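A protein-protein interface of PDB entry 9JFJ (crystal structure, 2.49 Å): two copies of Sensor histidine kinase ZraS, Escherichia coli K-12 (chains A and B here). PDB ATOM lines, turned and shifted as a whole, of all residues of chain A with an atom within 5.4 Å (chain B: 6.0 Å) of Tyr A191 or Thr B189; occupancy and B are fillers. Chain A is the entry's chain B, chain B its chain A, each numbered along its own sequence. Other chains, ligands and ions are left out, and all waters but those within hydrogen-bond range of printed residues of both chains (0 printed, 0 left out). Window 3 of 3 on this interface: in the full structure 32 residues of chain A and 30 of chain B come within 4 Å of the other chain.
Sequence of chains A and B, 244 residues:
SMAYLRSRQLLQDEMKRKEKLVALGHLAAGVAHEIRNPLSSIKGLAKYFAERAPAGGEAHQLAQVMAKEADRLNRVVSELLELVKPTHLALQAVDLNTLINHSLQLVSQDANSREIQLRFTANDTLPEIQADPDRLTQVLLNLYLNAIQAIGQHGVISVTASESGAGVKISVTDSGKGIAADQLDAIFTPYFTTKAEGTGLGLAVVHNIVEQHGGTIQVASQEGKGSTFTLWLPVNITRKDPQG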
ATOM      1  N   ALA A  23     -16.470  -7.017 -28.662  1.00  0.00           N
ATOM      2  CA  ALA A  23     -15.599  -7.237 -27.496  1.00  0.00           C
ATOM      3  C   ALA A  23     -14.247  -7.776 -27.946  1.00  0.00           C
ATOM      4  O   ALA A  23     -13.230  -7.364 -27.389  1.00  0.00           O
ATOM      5  CB  ALA A  23     -16.279  -8.202 -26.586  1.00  0.00           C
ATOM      6  N   LEU A  24     -14.253  -8.709 -28.890  1.00  0.00           N
ATOM      7  CA  LEU A  24     -12.991  -9.315 -29.355  1.00  0.00           C
ATOM      8  C   LEU A  24     -12.172  -8.236 -30.027  1.00  0.00           C
ATOM      9  O   LEU A  24     -10.959  -8.225 -29.857  1.00  0.00           O
ATOM     10  CB  LEU A  24     -13.290 -10.470 -30.306  1.00  0.00           C
ATOM     11  CG  LEU A  24     -13.189 -11.870 -29.709  1.00  0.00           C
ATOM     12  CD1 LEU A  24     -14.009 -11.988 -28.435  1.00  0.00           C
ATOM     13  CD2 LEU A  24     -13.635 -12.914 -30.717  1.00  0.00           C
ATOM     14  N   HIS A  26     -12.092  -5.031 -29.228  1.00  0.00           N
ATOM     15  CA  HIS A  26     -11.514  -4.202 -28.150  1.00  0.00           C
ATOM     16  C   HIS A  26     -10.372  -4.950 -27.488  1.00  0.00           C
ATOM     17  O   HIS A  26      -9.308  -4.357 -27.295  1.00  0.00           O
ATOM     18  CB  HIS A  26     -12.610  -3.867 -27.137  1.00  0.00           C
ATOM     19  CG  HIS A  26     -12.143  -3.085 -25.955  1.00  0.00           C
ATOM     20  ND1 HIS A  26     -11.792  -1.755 -26.042  1.00  0.00           N
ATOM     21  CD2 HIS A  26     -11.989  -3.433 -24.660  1.00  0.00           C
ATOM     22  CE1 HIS A  26     -11.435  -1.324 -24.855  1.00  0.00           C
ATOM     23  NE2 HIS A  26     -11.546  -2.331 -23.991  1.00  0.00           N
ATOM     24  N   LEU A  27     -10.586  -6.224 -27.200  1.00  0.00           N
ATOM     25  CA  LEU A  27      -9.539  -6.970 -26.496  1.00  0.00           C
ATOM     26  C   LEU A  27      -8.308  -6.964 -27.402  1.00  0.00           C
ATOM     27  O   LEU A  27      -7.201  -6.689 -26.921  1.00  0.00           O
ATOM     28  CB  LEU A  27     -10.075  -8.373 -26.224  1.00  0.00           C
ATOM     29  CG  LEU A  27     -11.091  -8.493 -25.093  1.00  0.00           C
ATOM     30  CD1 LEU A  27     -11.812  -9.825 -25.168  1.00  0.00           C
ATOM     31  CD2 LEU A  27     -10.416  -8.336 -23.743  1.00  0.00           C
ATOM     32  N   THR A 189     -17.723   3.826 -24.168  1.00  0.00           N
ATOM     33  CA  THR A 189     -16.562   2.956 -24.047  1.00  0.00           C
ATOM     34  C   THR A 189     -17.009   1.515 -23.826  1.00  0.00           C
ATOM     35  O   THR A 189     -17.891   1.269 -23.000  1.00  0.00           O
ATOM     36  CB  THR A 189     -15.665   3.412 -22.902  1.00  0.00           C
ATOM     37  OG1 THR A 189     -16.390   3.336 -21.668  1.00  0.00           O
ATOM     38  CG2 THR A 189     -15.201   4.843 -23.124  1.00  0.00           C
ATOM     39  N   PRO A 190     -16.436   0.553 -24.547  1.00  0.00           N
ATOM     40  CA  PRO A 190     -16.825  -0.847 -24.345  1.00  0.00           C
ATOM     41  C   PRO A 190     -16.559  -1.307 -22.921  1.00  0.00           C
ATOM     42  O   PRO A 190     -15.614  -0.853 -22.270  1.00  0.00           O
ATOM     43  CB  PRO A 190     -15.953  -1.602 -25.352  1.00  0.00           C
ATOM     44  CG  PRO A 190     -15.620  -0.589 -26.397  1.00  0.00           C
ATOM     45  CD  PRO A 190     -15.481   0.705 -25.657  1.00  0.00           C
ATOM     46  N   TYR A 191     -17.430  -2.195 -22.440  1.00  0.00           N
ATOM     47  CA  TYR A 191     -17.413  -2.776 -21.101  1.00  0.00           C
ATOM     48  C   TYR A 191     -17.811  -1.768 -20.034  1.00  0.00           C
ATOM     49  O   TYR A 191     -17.562  -2.015 -18.847  1.00  0.00           O
ATOM     50  CB  TYR A 191     -16.027  -3.343 -20.791  1.00  0.00           C
ATOM     51  CG  TYR A 191     -15.623  -4.501 -21.673  1.00  0.00           C
ATOM     52  CD1 TYR A 191     -15.974  -5.809 -21.344  1.00  0.00           C
ATOM     53  CD2 TYR A 191     -14.893  -4.292 -22.832  1.00  0.00           C
ATOM     54  CE1 TYR A 191     -15.606  -6.869 -22.150  1.00  0.00           C
ATOM     55  CE2 TYR A 191     -14.520  -5.346 -23.643  1.00  0.00           C
ATOM     56  CZ  TYR A 191     -14.883  -6.634 -23.297  1.00  0.00           C
ATOM     57  OH  TYR A 191     -14.514  -7.688 -24.101  1.00  0.00           O
ATOM     58  N   PHE A 192     -18.394  -0.636 -20.444  1.00  0.00           N
ATOM     59  CA  PHE A 192     -18.892   0.372 -19.468  1.00  0.00           C
ATOM     60  C   PHE A 192     -20.397   0.200 -19.256  1.00  0.00           C
ATOM     61  O   PHE A 192     -21.130   0.297 -20.245  1.00  0.00           O
ATOM     62  CB  PHE A 192     -18.597   1.795 -19.940  1.00  0.00           C
ATOM     63  CG  PHE A 192     -18.914   2.871 -18.931  1.00  0.00           C
ATOM     64  CD1 PHE A 192     -20.192   3.390 -18.817  1.00  0.00           C
ATOM     65  CD2 PHE A 192     -17.922   3.376 -18.109  1.00  0.00           C
ATOM     66  CE1 PHE A 192     -20.471   4.383 -17.894  1.00  0.00           C
ATOM     67  CE2 PHE A 192     -18.206   4.368 -17.185  1.00  0.00           C
ATOM     68  CZ  PHE A 192     -19.480   4.868 -17.079  1.00  0.00           C
ATOM     69  N   THR A 193     -20.827   0.020 -18.008  1.00  0.00           N
ATOM     70  CA  THR A 193     -22.256  -0.217 -17.707  1.00  0.00           C
ATOM     71  C   THR A 193     -22.576   0.249 -16.292  1.00  0.00           C
ATOM     72  O   THR A 193     -21.668   0.239 -15.460  1.00  0.00           O
ATOM     73  CB  THR A 193     -22.617  -1.696 -17.848  1.00  0.00           C
ATOM     74  OG1 THR A 193     -23.885  -1.899 -17.225  1.00  0.00           O
ATOM     75  CG2 THR A 193     -21.599  -2.618 -17.219  1.00  0.00           C
ATOM     76  N   GLY A 200     -21.297  -4.314 -21.269  1.00  0.00           N
ATOM     77  CA  GLY A 200     -21.188  -2.864 -21.488  1.00  0.00           C
ATOM     78  C   GLY A 200     -20.938  -2.665 -22.951  1.00  0.00           C
ATOM     79  O   GLY A 200     -20.158  -1.779 -23.304  1.00  0.00           O
ATOM     80  N   LEU A 201     -21.555  -3.503 -23.776  1.00  0.00           N
ATOM     81  CA  LEU A 201     -21.199  -3.464 -25.210  1.00  0.00           C
ATOM     82  C   LEU A 201     -22.275  -2.893 -26.137  1.00  0.00           C
ATOM     83  O   LEU A 201     -21.941  -2.680 -27.300  1.00  0.00           O
ATOM     84  CB  LEU A 201     -20.831  -4.895 -25.593  1.00  0.00           C
ATOM     85  CG  LEU A 201     -19.595  -5.454 -24.890  1.00  0.00           C
ATOM     86  CD1 LEU A 201     -19.572  -6.972 -24.953  1.00  0.00           C
ATOM     87  CD2 LEU A 201     -18.322  -4.871 -25.479  1.00  0.00           C
ATOM     88  N   ASP B 185     -15.957   1.379 -11.307  1.00  0.00           N
ATOM     89  CA  ASP B 185     -16.591   0.831 -12.497  1.00  0.00           C
ATOM     90  C   ASP B 185     -15.609   0.332 -13.544  1.00  0.00           C
ATOM     91  O   ASP B 185     -15.906  -0.647 -14.231  1.00  0.00           O
ATOM     92  CB  ASP B 185     -17.510   1.871 -13.143  1.00  0.00           C
ATOM     93  CG  ASP B 185     -16.840   3.215 -13.311  1.00  0.00           C
ATOM     94  OD1 ASP B 185     -16.573   3.877 -12.290  1.00  0.00           O
ATOM     95  OD2 ASP B 185     -16.568   3.601 -14.467  1.00  0.00           O
ATOM     96  N   ALA B 186     -14.450   0.970 -13.677  1.00  0.00           N
ATOM     97  CA  ALA B 186     -13.412   0.486 -14.581  1.00  0.00           C
ATOM     98  C   ALA B 186     -12.650  -0.701 -14.005  1.00  0.00           C
ATOM     99  O   ALA B 186     -11.775  -1.248 -14.684  1.00  0.00           O
ATOM    100  CB  ALA B 186     -12.437   1.611 -14.921  1.00  0.00           C
ATOM    101  N   ILE B 187     -12.963  -1.101 -12.774  1.00  0.00           N
ATOM    102  CA  ILE B 187     -12.256  -2.185 -12.111  1.00  0.00           C
ATOM    103  C   ILE B 187     -12.399  -3.505 -12.855  1.00  0.00           C
ATOM    104  O   ILE B 187     -11.439  -4.281 -12.919  1.00  0.00           O
ATOM    105  CB  ILE B 187     -12.756  -2.269 -10.652  1.00  0.00           C
ATOM    106  CG1 ILE B 187     -12.063  -3.393  -9.893  1.00  0.00           C
ATOM    107  CG2 ILE B 187     -14.268  -2.409 -10.604  1.00  0.00           C
ATOM    108  CD1 ILE B 187     -12.678  -3.660  -8.546  1.00  0.00           C
ATOM    109  N   PHE B 188     -13.524  -3.723 -13.519  1.00  0.00           N
ATOM    110  CA  PHE B 188     -13.739  -4.984 -14.258  1.00  0.00           C
ATOM    111  C   PHE B 188     -13.396  -4.767 -15.727  1.00  0.00           C
ATOM    112  O   PHE B 188     -13.500  -5.721 -16.488  1.00  0.00           O
ATOM    113  CB  PHE B 188     -15.182  -5.457 -14.112  1.00  0.00           C
ATOM    114  CG  PHE B 188     -15.573  -5.987 -12.764  1.00  0.00           C
ATOM    115  CD1 PHE B 188     -15.276  -7.287 -12.404  1.00  0.00           C
ATOM    116  CD2 PHE B 188     -16.276  -5.198 -11.874  1.00  0.00           C
ATOM    117  CE1 PHE B 188     -15.655  -7.776 -11.170  1.00  0.00           C
ATOM    118  CE2 PHE B 188     -16.648  -5.691 -10.636  1.00  0.00           C
ATOM    119  CZ  PHE B 188     -16.339  -6.976 -10.286  1.00  0.00           C
ATOM    120  N   THR B 189     -13.022  -3.540 -16.100  1.00  0.00           N
ATOM    121  CA  THR B 189     -12.739  -3.258 -17.495  1.00  0.00           C
ATOM    122  C   THR B 189     -11.443  -3.951 -17.913  1.00  0.00           C
ATOM    123  O   THR B 189     -10.453  -3.915 -17.178  1.00  0.00           O
ATOM    124  CB  THR B 189     -12.638  -1.756 -17.732  1.00  0.00           C
ATOM    125  OG1 THR B 189     -13.924  -1.155 -17.529  1.00  0.00           O
ATOM    126  CG2 THR B 189     -12.169  -1.453 -19.142  1.00  0.00           C
ATOM    127  N   PRO B 190     -11.421  -4.596 -19.075  1.00  0.00           N
ATOM    128  CA  PRO B 190     -10.196  -5.240 -19.543  1.00  0.00           C
ATOM    129  C   PRO B 190      -9.050  -4.253 -19.702  1.00  0.00           C
ATOM    130  O   PRO B 190      -9.244  -3.108 -20.113  1.00  0.00           O
ATOM    131  CB  PRO B 190     -10.607  -5.830 -20.895  1.00  0.00           C
ATOM    132  CG  PRO B 190     -12.056  -6.094 -20.740  1.00  0.00           C
ATOM    133  CD  PRO B 190     -12.586  -4.978 -19.888  1.00  0.00           C
ATOM    134  N   TYR B 191      -7.848  -4.719 -19.359  1.00  0.00           N
ATOM    135  CA  TYR B 191      -6.576  -4.024 -19.533  1.00  0.00           C
ATOM    136  C   TYR B 191      -6.391  -2.858 -18.573  1.00  0.00           C
ATOM    137  O   TYR B 191      -5.467  -2.058 -18.756  1.00  0.00           O
ATOM    138  CB  TYR B 191      -6.387  -3.544 -20.976  1.00  0.00           C
ATOM    139  CG  TYR B 191      -6.401  -4.666 -21.983  1.00  0.00           C
ATOM    140  CD1 TYR B 191      -5.411  -5.636 -21.980  1.00  0.00           C
ATOM    141  CD2 TYR B 191      -7.413  -4.763 -22.922  1.00  0.00           C
ATOM    142  CE1 TYR B 191      -5.428  -6.664 -22.890  1.00  0.00           C
ATOM    143  CE2 TYR B 191      -7.438  -5.783 -23.833  1.00  0.00           C
ATOM    144  CZ  TYR B 191      -6.441  -6.736 -23.815  1.00  0.00           C
ATOM    145  OH  TYR B 191      -6.464  -7.758 -24.728  1.00  0.00           O
ATOM    146  N   PHE B 192      -7.227  -2.741 -17.547  1.00  0.00           N
ATOM    147  CA  PHE B 192      -7.121  -1.671 -16.566  1.00  0.00           C
ATOM    148  C   PHE B 192      -6.439  -2.196 -15.317  1.00  0.00           C
ATOM    149  O   PHE B 192      -6.922  -3.145 -14.690  1.00  0.00           O
ATOM    150  CB  PHE B 192      -8.498  -1.112 -16.209  1.00  0.00           C
ATOM    151  CG  PHE B 192      -8.469  -0.127 -15.077  1.00  0.00           C
ATOM    152  CD1 PHE B 192      -7.944   1.137 -15.262  1.00  0.00           C
ATOM    153  CD2 PHE B 192      -8.941  -0.471 -13.822  1.00  0.00           C
ATOM    154  CE1 PHE B 192      -7.905   2.043 -14.224  1.00  0.00           C
ATOM    155  CE2 PHE B 192      -8.905   0.434 -12.779  1.00  0.00           C
ATOM    156  CZ  PHE B 192      -8.387   1.694 -12.984  1.00  0.00           C
ATOM    157  N   GLY B 200      -4.451  -6.274 -16.663  1.00  0.00           N
ATOM    158  CA  GLY B 200      -5.782  -5.832 -16.241  1.00  0.00           C
ATOM    159  C   GLY B 200      -6.830  -6.757 -16.781  1.00  0.00           C
ATOM    160  O   GLY B 200      -7.802  -6.269 -17.337  1.00  0.00           O
ATOM    161  N   LEU B 201      -6.679  -8.044 -16.545  1.00  0.00           N
ATOM    162  CA  LEU B 201      -7.591  -8.995 -17.199  1.00  0.00           C
ATOM    163  C   LEU B 201      -7.953 -10.073 -16.201  1.00  0.00           C
ATOM    164  O   LEU B 201      -8.664 -10.992 -16.571  1.00  0.00           O
ATOM    165  CB  LEU B 201      -6.866  -9.582 -18.415  1.00  0.00           C
ATOM    166  CG  LEU B 201      -6.555  -8.630 -19.564  1.00  0.00           C
ATOM    167  CD1 LEU B 201      -5.619  -9.286 -20.557  1.00  0.00           C
ATOM    168  CD2 LEU B 201      -7.827  -8.184 -20.260  1.00  0.00           C
ATOM    169  N   ALA B 204     -11.518  -9.392 -15.543  1.00  0.00           N
ATOM    170  CA  ALA B 204     -12.195  -9.729 -16.793  1.00  0.00           C
ATOM    171  C   ALA B 204     -12.417 -11.234 -16.895  1.00  0.00           C
ATOM    172  O   ALA B 204     -13.505 -11.690 -17.264  1.00  0.00           O
ATOM    173  CB  ALA B 204     -11.388  -9.221 -17.985  1.00  0.00           C
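O of Gly A200 lies within hydrogen-bond range of N of Tyr A191 (2.9 Å). O of Gly B200 is in hydrogen-bond range of N of Tyr B191 (2.5 Å).
Of the printed residues of chain B, Leu A27 touches Pro B190 and Tyr B191. Tyr A191 touches just these residues of chain B: Thr B189 (3.96 Å) and Pro B190 (3.6 Å). Of the printed residues of chain B, Phe A192 touches Asp B185. Ile B187 touches none of the printed residues of chain A. Of chain A, only Tyr A191 (3.96 Å) comes within 4 Å of Thr B189. Of the printed residues of chain A, Tyr B191 touches Leu A27.
Among the printed residues, merely in contact across the chains: Phe A192 with Asp B185, Tyr A191 with Pro B190, Leu A27 with Pro B190 and Tyr A191 with Thr B189.
The side-chain hydroxyl (OH) of Tyr B191 is in hydrogen-bond range of the backbone carbonyl oxygen (O) of Leu A27.
Of the 11 printed residues of chain A, 3 touch a printed residue of chain B. Printed residues of chain A that touch a printed residue of chain B: Leu A27, Tyr A191 and Phe A192. Along chain A the printed residues that touch a printed residue of chain B span positions 27 to 192. Hydrophobic or aromatic side chains of chain B within 4 Å of the printed part of chain A: Pro B190 and Tyr B191. Among the printed residues, no Asp or Glu carboxylate lies within 4 Å of a Lys or Arg side-chain nitrogen of the other chain.
Tyr A191 touches Thr B189, but with the chains exchanged Thr A189 does not touch Tyr B191 (11.5 Å). Tyr A191 touches Pro B190, but with the chains exchanged Pro A190 does not touch Tyr B191 (9.1 Å). 6 positions are printed for both chains.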
